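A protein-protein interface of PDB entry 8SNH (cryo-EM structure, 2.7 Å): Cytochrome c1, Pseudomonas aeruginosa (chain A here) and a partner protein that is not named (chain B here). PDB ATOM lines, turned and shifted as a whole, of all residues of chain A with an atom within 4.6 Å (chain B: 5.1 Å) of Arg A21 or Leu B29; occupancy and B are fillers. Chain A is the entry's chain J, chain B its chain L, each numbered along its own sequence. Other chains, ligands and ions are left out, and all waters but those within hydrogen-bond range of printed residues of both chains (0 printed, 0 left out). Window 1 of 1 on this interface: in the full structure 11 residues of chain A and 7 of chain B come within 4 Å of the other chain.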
ATOM      1  N   GLN A  17       9.867 -17.361  13.352  1.00  0.00           N
ATOM      2  CA  GLN A  17       8.419 -17.255  13.482  1.00  0.00           C
ATOM      3  C   GLN A  17       7.998 -15.825  13.787  1.00  0.00           C
ATOM      4  O   GLN A  17       7.039 -15.311  13.196  1.00  0.00           O
ATOM      5  CB  GLN A  17       7.928 -18.201  14.576  1.00  0.00           C
ATOM      6  CG  GLN A  17       7.826 -19.649  14.139  1.00  0.00           C
ATOM      7  CD  GLN A  17       7.975 -20.615  15.296  1.00  0.00           C
ATOM      8  OE1 GLN A  17       7.804 -20.242  16.455  1.00  0.00           O
ATOM      9  NE2 GLN A  17       8.300 -21.863  14.986  1.00  0.00           N
ATOM     10  N   ASP A  18       8.702 -15.165  14.708  1.00  0.00           N
ATOM     11  CA  ASP A  18       8.395 -13.769  14.998  1.00  0.00           C
ATOM     12  C   ASP A  18       8.628 -12.898  13.770  1.00  0.00           C
ATOM     13  O   ASP A  18       7.843 -11.985  13.486  1.00  0.00           O
ATOM     14  CB  ASP A  18       9.235 -13.276  16.174  1.00  0.00           C
ATOM     15  CG  ASP A  18       8.921 -11.843  16.552  1.00  0.00           C
ATOM     16  OD1 ASP A  18       7.742 -11.547  16.835  1.00  0.00           O
ATOM     17  OD2 ASP A  18       9.852 -11.011  16.565  1.00  0.00           O
ATOM     18  N   GLY A  19       9.701 -13.168  13.028  1.00  0.00           N
ATOM     19  CA  GLY A  19       9.952 -12.419  11.808  1.00  0.00           C
ATOM     20  C   GLY A  19       8.873 -12.631  10.765  1.00  0.00           C
ATOM     21  O   GLY A  19       8.483 -11.696  10.067  1.00  0.00           O
ATOM     22  N   ALA A  20       8.386 -13.865  10.638  1.00  0.00           N
ATOM     23  CA  ALA A  20       7.307 -14.148   9.700  1.00  0.00           C
ATOM     24  C   ALA A  20       6.031 -13.427  10.103  1.00  0.00           C
ATOM     25  O   ALA A  20       5.309 -12.907   9.248  1.00  0.00           O
ATOM     26  CB  ALA A  20       7.065 -15.654   9.618  1.00  0.00           C
ATOM     27  N   ARG A  21       5.728 -13.399  11.401  1.00  0.00           N
ATOM     28  CA  ARG A  21       4.564 -12.657  11.876  1.00  0.00           C
ATOM     29  C   ARG A  21       4.703 -11.171  11.561  1.00  0.00           C
ATOM     30  O   ARG A  21       3.763 -10.533  11.063  1.00  0.00           O
ATOM     31  CB  ARG A  21       4.391 -12.894  13.377  1.00  0.00           C
ATOM     32  CG  ARG A  21       3.224 -12.165  14.017  1.00  0.00           C
ATOM     33  CD  ARG A  21       3.705 -11.156  15.044  1.00  0.00           C
ATOM     34  NE  ARG A  21       2.642 -10.741  15.951  1.00  0.00           N
ATOM     35  CZ  ARG A  21       2.705  -9.678  16.741  1.00  0.00           C
ATOM     36  NH1 ARG A  21       3.774  -8.900  16.769  1.00  0.00           N
ATOM     37  NH2 ARG A  21       1.669  -9.389  17.524  1.00  0.00           N
ATOM     38  N   THR A  22       5.884 -10.609  11.825  1.00  0.00           N
ATOM     39  CA  THR A  22       6.125  -9.206  11.510  1.00  0.00           C
ATOM     40  C   THR A  22       5.972  -8.943  10.018  1.00  0.00           C
ATOM     41  O   THR A  22       5.376  -7.940   9.616  1.00  0.00           O
ATOM     42  CB  THR A  22       7.520  -8.797  11.983  1.00  0.00           C
ATOM     43  OG1 THR A  22       7.632  -9.013  13.395  1.00  0.00           O
ATOM     44  CG2 THR A  22       7.786  -7.334  11.674  1.00  0.00           C
ATOM     45  N   PHE A  23       6.514  -9.825   9.180  1.00  0.00           N
ATOM     46  CA  PHE A  23       6.398  -9.648   7.739  1.00  0.00           C
ATOM     47  C   PHE A  23       4.945  -9.728   7.290  1.00  0.00           C
ATOM     48  O   PHE A  23       4.496  -8.922   6.468  1.00  0.00           O
ATOM     49  CB  PHE A  23       7.241 -10.697   7.017  1.00  0.00           C
ATOM     50  CG  PHE A  23       7.338 -10.483   5.538  1.00  0.00           C
ATOM     51  CD1 PHE A  23       8.300  -9.641   5.011  1.00  0.00           C
ATOM     52  CD2 PHE A  23       6.470 -11.123   4.673  1.00  0.00           C
ATOM     53  CE1 PHE A  23       8.390  -9.441   3.651  1.00  0.00           C
ATOM     54  CE2 PHE A  23       6.556 -10.925   3.313  1.00  0.00           C
ATOM     55  CZ  PHE A  23       7.518 -10.084   2.801  1.00  0.00           C
ATOM     56  N   ALA A  24       4.191 -10.688   7.825  1.00  0.00           N
ATOM     57  CA  ALA A  24       2.812 -10.873   7.396  1.00  0.00           C
ATOM     58  C   ALA A  24       1.925  -9.721   7.837  1.00  0.00           C
ATOM     59  O   ALA A  24       0.931  -9.419   7.168  1.00  0.00           O
ATOM     60  CB  ALA A  24       2.266 -12.192   7.941  1.00  0.00           C
ATOM     61  N   ASN A  25       2.255  -9.070   8.953  1.00  0.00           N
ATOM     62  CA  ASN A  25       1.397  -8.009   9.472  1.00  0.00           C
ATOM     63  C   ASN A  25       1.817  -6.624   8.983  1.00  0.00           C
ATOM     64  O   ASN A  25       0.984  -5.857   8.490  1.00  0.00           O
ATOM     65  CB  ASN A  25       1.388  -8.057  11.003  1.00  0.00           C
ATOM     66  CG  ASN A  25       0.536  -9.186  11.537  1.00  0.00           C
ATOM     67  OD1 ASN A  25      -0.686  -9.076  11.603  1.00  0.00           O
ATOM     68  ND2 ASN A  25       1.176 -10.282  11.914  1.00  0.00           N
ATOM     69  N   ILE A  47       5.938 -24.313  11.816  1.00  0.00           N
ATOM     70  CA  ILE A  47       4.596 -23.839  12.142  1.00  0.00           C
ATOM     71  C   ILE A  47       3.582 -24.869  11.656  1.00  0.00           C
ATOM     72  O   ILE A  47       3.634 -25.275  10.487  1.00  0.00           O
ATOM     73  CB  ILE A  47       4.325 -22.461  11.519  1.00  0.00           C
ATOM     74  CG1 ILE A  47       5.300 -21.419  12.072  1.00  0.00           C
ATOM     75  CG2 ILE A  47       2.893 -22.031  11.786  1.00  0.00           C
ATOM     76  CD1 ILE A  47       5.517 -20.239  11.151  1.00  0.00           C
ATOM     77  N   LEU A  51      -2.096 -23.629  12.007  1.00  0.00           N
ATOM     78  CA  LEU A  51      -1.642 -22.395  12.638  1.00  0.00           C
ATOM     79  C   LEU A  51      -1.165 -21.389  11.600  1.00  0.00           C
ATOM     80  O   LEU A  51      -1.447 -20.190  11.712  1.00  0.00           O
ATOM     81  CB  LEU A  51      -0.531 -22.706  13.639  1.00  0.00           C
ATOM     82  CG  LEU A  51      -0.466 -21.783  14.853  1.00  0.00           C
ATOM     83  CD1 LEU A  51      -1.572 -22.114  15.842  1.00  0.00           C
ATOM     84  CD2 LEU A  51       0.895 -21.888  15.510  1.00  0.00           C
ATOM     85  N   LYS A  55      -2.920 -17.733  11.274  1.00  0.00           N
ATOM     86  CA  LYS A  55      -2.150 -16.637  11.844  1.00  0.00           C
ATOM     87  C   LYS A  55      -1.380 -15.807  10.830  1.00  0.00           C
ATOM     88  O   LYS A  55      -1.204 -14.608  11.051  1.00  0.00           O
ATOM     89  CB  LYS A  55      -1.157 -17.177  12.881  1.00  0.00           C
ATOM     90  CG  LYS A  55      -1.788 -18.035  13.966  1.00  0.00           C
ATOM     91  CD  LYS A  55      -2.125 -17.219  15.202  1.00  0.00           C
ATOM     92  CE  LYS A  55      -3.332 -17.786  15.928  1.00  0.00           C
ATOM     93  NZ  LYS A  55      -3.353 -17.410  17.368  1.00  0.00           N
ATOM     94  N   LEU A  56      -0.912 -16.401   9.731  1.00  0.00           N
ATOM     95  CA  LEU A  56      -0.047 -15.696   8.796  1.00  0.00           C
ATOM     96  C   LEU A  56      -0.645 -15.496   7.412  1.00  0.00           C
ATOM     97  O   LEU A  56      -0.175 -14.613   6.688  1.00  0.00           O
ATOM     98  CB  LEU A  56       1.294 -16.433   8.647  1.00  0.00           C
ATOM     99  CG  LEU A  56       2.167 -16.450   9.906  1.00  0.00           C
ATOM    100  CD1 LEU A  56       3.389 -17.331   9.714  1.00  0.00           C
ATOM    101  CD2 LEU A  56       2.584 -15.045  10.291  1.00  0.00           C
ATOM    102  N   LYS A 187      13.044  -7.157  17.313  1.00  0.00           N
ATOM    103  CA  LYS A 187      11.989  -7.284  16.312  1.00  0.00           C
ATOM    104  C   LYS A 187      12.569  -7.230  14.904  1.00  0.00           C
ATOM    105  O   LYS A 187      12.256  -8.070  14.050  1.00  0.00           O
ATOM    106  CB  LYS A 187      10.955  -6.173  16.512  1.00  0.00           C
ATOM    107  CG  LYS A 187       9.722  -6.273  15.624  1.00  0.00           C
ATOM    108  CD  LYS A 187       8.835  -7.456  15.989  1.00  0.00           C
ATOM    109  CE  LYS A 187       8.157  -7.263  17.338  1.00  0.00           C
ATOM    110  NZ  LYS A 187       7.211  -8.368  17.655  1.00  0.00           N
ATOM    111  N   ILE B  25       3.972 -21.320  19.617  1.00  0.00           N
ATOM    112  CA  ILE B  25       4.005 -20.787  18.260  1.00  0.00           C
ATOM    113  C   ILE B  25       2.804 -19.882  18.021  1.00  0.00           C
ATOM    114  O   ILE B  25       2.925 -18.813  17.412  1.00  0.00           O
ATOM    115  CB  ILE B  25       4.064 -21.932  17.229  1.00  0.00           C
ATOM    116  CG1 ILE B  25       5.246 -22.865  17.506  1.00  0.00           C
ATOM    117  CG2 ILE B  25       4.187 -21.373  15.818  1.00  0.00           C
ATOM    118  CD1 ILE B  25       5.063 -24.254  16.935  1.00  0.00           C
ATOM    119  N   ALA B  26       1.625 -20.294  18.496  1.00  0.00           N
ATOM    120  CA  ALA B  26       0.419 -19.504  18.271  1.00  0.00           C
ATOM    121  C   ALA B  26       0.542 -18.121  18.898  1.00  0.00           C
ATOM    122  O   ALA B  26       0.172 -17.116  18.279  1.00  0.00           O
ATOM    123  CB  ALA B  26      -0.799 -20.237  18.831  1.00  0.00           C
ATOM    124  N   LYS B  27       1.058 -18.049  20.125  1.00  0.00           N
ATOM    125  CA  LYS B  27       1.298 -16.751  20.746  1.00  0.00           C
ATOM    126  C   LYS B  27       2.324 -15.955  19.952  1.00  0.00           C
ATOM    127  O   LYS B  27       2.178 -14.740  19.773  1.00  0.00           O
ATOM    128  CB  LYS B  27       1.767 -16.943  22.188  1.00  0.00           C
ATOM    129  CG  LYS B  27       0.653 -17.294  23.163  1.00  0.00           C
ATOM    130  CD  LYS B  27       1.058 -17.015  24.605  1.00  0.00           C
ATOM    131  CE  LYS B  27       1.114 -18.291  25.432  1.00  0.00           C
ATOM    132  NZ  LYS B  27       2.382 -19.040  25.213  1.00  0.00           N
ATOM    133  N   ARG B  28       3.371 -16.626  19.473  1.00  0.00           N
ATOM    134  CA  ARG B  28       4.393 -15.957  18.677  1.00  0.00           C
ATOM    135  C   ARG B  28       3.816 -15.383  17.391  1.00  0.00           C
ATOM    136  O   ARG B  28       4.298 -14.356  16.898  1.00  0.00           O
ATOM    137  CB  ARG B  28       5.513 -16.947  18.355  1.00  0.00           C
ATOM    138  CG  ARG B  28       6.867 -16.319  18.080  1.00  0.00           C
ATOM    139  CD  ARG B  28       7.984 -17.145  18.704  1.00  0.00           C
ATOM    140  NE  ARG B  28       7.788 -18.574  18.479  1.00  0.00           N
ATOM    141  CZ  ARG B  28       7.972 -19.524  19.388  1.00  0.00           C
ATOM    142  NH1 ARG B  28       8.380 -19.244  20.616  1.00  0.00           N
ATOM    143  NH2 ARG B  28       7.740 -20.790  19.057  1.00  0.00           N
ATOM    144  N   LEU B  29       2.789 -16.024  16.838  1.00  0.00           N
ATOM    145  CA  LEU B  29       2.266 -15.701  15.518  1.00  0.00           C
ATOM    146  C   LEU B  29       0.991 -14.865  15.572  1.00  0.00           C
ATOM    147  O   LEU B  29       0.339 -14.687  14.538  1.00  0.00           O
ATOM    148  CB  LEU B  29       2.009 -16.993  14.741  1.00  0.00           C
ATOM    149  CG  LEU B  29       3.061 -17.421  13.719  1.00  0.00           C
ATOM    150  CD1 LEU B  29       4.460 -17.354  14.303  1.00  0.00           C
ATOM    151  CD2 LEU B  29       2.753 -18.826  13.226  1.00  0.00           C
ATOM    152  N   GLU B  30       0.631 -14.342  16.737  1.00  0.00           N
ATOM    153  CA  GLU B  30      -0.636 -13.637  16.881  1.00  0.00           C
ATOM    154  C   GLU B  30      -0.676 -12.447  15.923  1.00  0.00           C
ATOM    155  O   GLU B  30       0.293 -11.677  15.864  1.00  0.00           O
ATOM    156  CB  GLU B  30      -0.798 -13.150  18.323  1.00  0.00           C
ATOM    157  CG  GLU B  30      -1.641 -14.027  19.262  1.00  0.00           C
ATOM    158  CD  GLU B  30      -3.055 -14.320  18.775  1.00  0.00           C
ATOM    159  OE1 GLU B  30      -3.898 -14.690  19.621  1.00  0.00           O
ATOM    160  OE2 GLU B  30      -3.341 -14.183  17.573  1.00  0.00           O
ATOM    161  N   PRO B  31      -1.757 -12.255  15.161  1.00  0.00           N
ATOM    162  CA  PRO B  31      -1.826 -11.078  14.287  1.00  0.00           C
ATOM    163  C   PRO B  31      -1.785  -9.784  15.084  1.00  0.00           C
ATOM    164  O   PRO B  31      -2.276  -9.703  16.212  1.00  0.00           O
ATOM    165  CB  PRO B  31      -3.165 -11.249  13.560  1.00  0.00           C
ATOM    166  CG  PRO B  31      -3.461 -12.694  13.642  1.00  0.00           C
ATOM    167  CD  PRO B  31      -2.918 -13.140  14.960  1.00  0.00           C
ATOM    168  N   VAL B  32      -1.182  -8.761  14.477  1.00  0.00           N
ATOM    169  CA  VAL B  32      -1.027  -7.476  15.153  1.00  0.00           C
ATOM    170  C   VAL B  32      -2.385  -6.823  15.376  1.00  0.00           C
ATOM    171  O   VAL B  32      -2.695  -6.360  16.479  1.00  0.00           O
ATOM    172  CB  VAL B  32      -0.090  -6.563  14.345  1.00  0.00           C
ATOM    173  CG1 VAL B  32      -0.107  -5.145  14.903  1.00  0.00           C
ATOM    174  CG2 VAL B  32       1.319  -7.125  14.343  1.00  0.00           C
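The backbone carbonyl oxygen of Arg A21 sits at hydrogen-bond distance from the side-chain amide nitrogen of Asn A25, at 2.7 Å.
Gly A19 touches none of the printed residues of chain B. Arg A21 touches just these residues of chain B: Arg B28 (3.7 Å), Leu B29 (3.8 Å), Glu B30 (2.5 Å) and Val B32 (3.8 Å). Printed residues of chain B within 4 Å of Asn A25: Pro B31 and Val B32. Printed residues of chain B within 4 Å of Lys A55: Ala B26, Leu B29, Glu B30 and Pro B31. Lys A187 touches none of the printed residues of chain B. Printed residues of chain A within 4 Å of Val B32: Arg A21 and Asn A25. The nearest residue of chain B that does not touch Arg A21 is Pro B31 (4.2 Å). The nearest residue of chain A that does not touch Leu B29 is Leu A51 (4.2 Å).
Among the printed residues, pairs that only touch across the chains: Gln A17 with Ile B25 (3.8 Å), Gln A17 with Leu B29 (3.5 Å), Arg A21 with Arg B28 (3.7 Å), Arg A21 with Leu B29 (3.8 Å), Arg A21 with Val B32 (3.8 Å), Asn A25 with Pro B31 (3.5 Å), Ile A47 with Ile B25 (3.9 Å), Ile A47 with Leu B29 (3.5 Å), Leu A51 with Ile B25 (3.3 Å), Leu A51 with Ala B26 (3.5 Å), Lys A55 with Ala B26 (3.7 Å), Lys A55 with Leu B29 (3.3 Å), Lys A55 with Pro B31 (3.9 Å) and Leu A56 with Leu B29 (3.9 Å).
Of the 8 printed residues of chain B, 7 touch a printed residue of chain A. Printed residues of chain B that touch a printed residue of chain A: Ile B25, Ala B26, Arg B28, Leu B29, Glu B30, Pro B31 and Val B32. Hydrophobic or aromatic side chains of chain B that line the printed part of chain A: Ile B25, Ala B26, Leu B29, Pro B31 and Val B32. Along chain B the printed residues that touch a printed residue of chain A span positions 25 to 32. Of the 14 printed residues of chain A, 7 touch a printed residue of chain B.
OE1 of Gln A17 is in hydrogen-bond range of NE of Arg B28 (2.6 Å). O of Glu B30 sits at hydrogen-bond distance from NE of Arg A21 (2.5 Å). OD1 of Asn A25 lies within hydrogen-bond range of N of Val B32. The side-chain amino group (NZ) of Lys A55 is in salt-bridge range of the side-chain carboxylate (OE2) of Glu B30 (3.2 Å).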
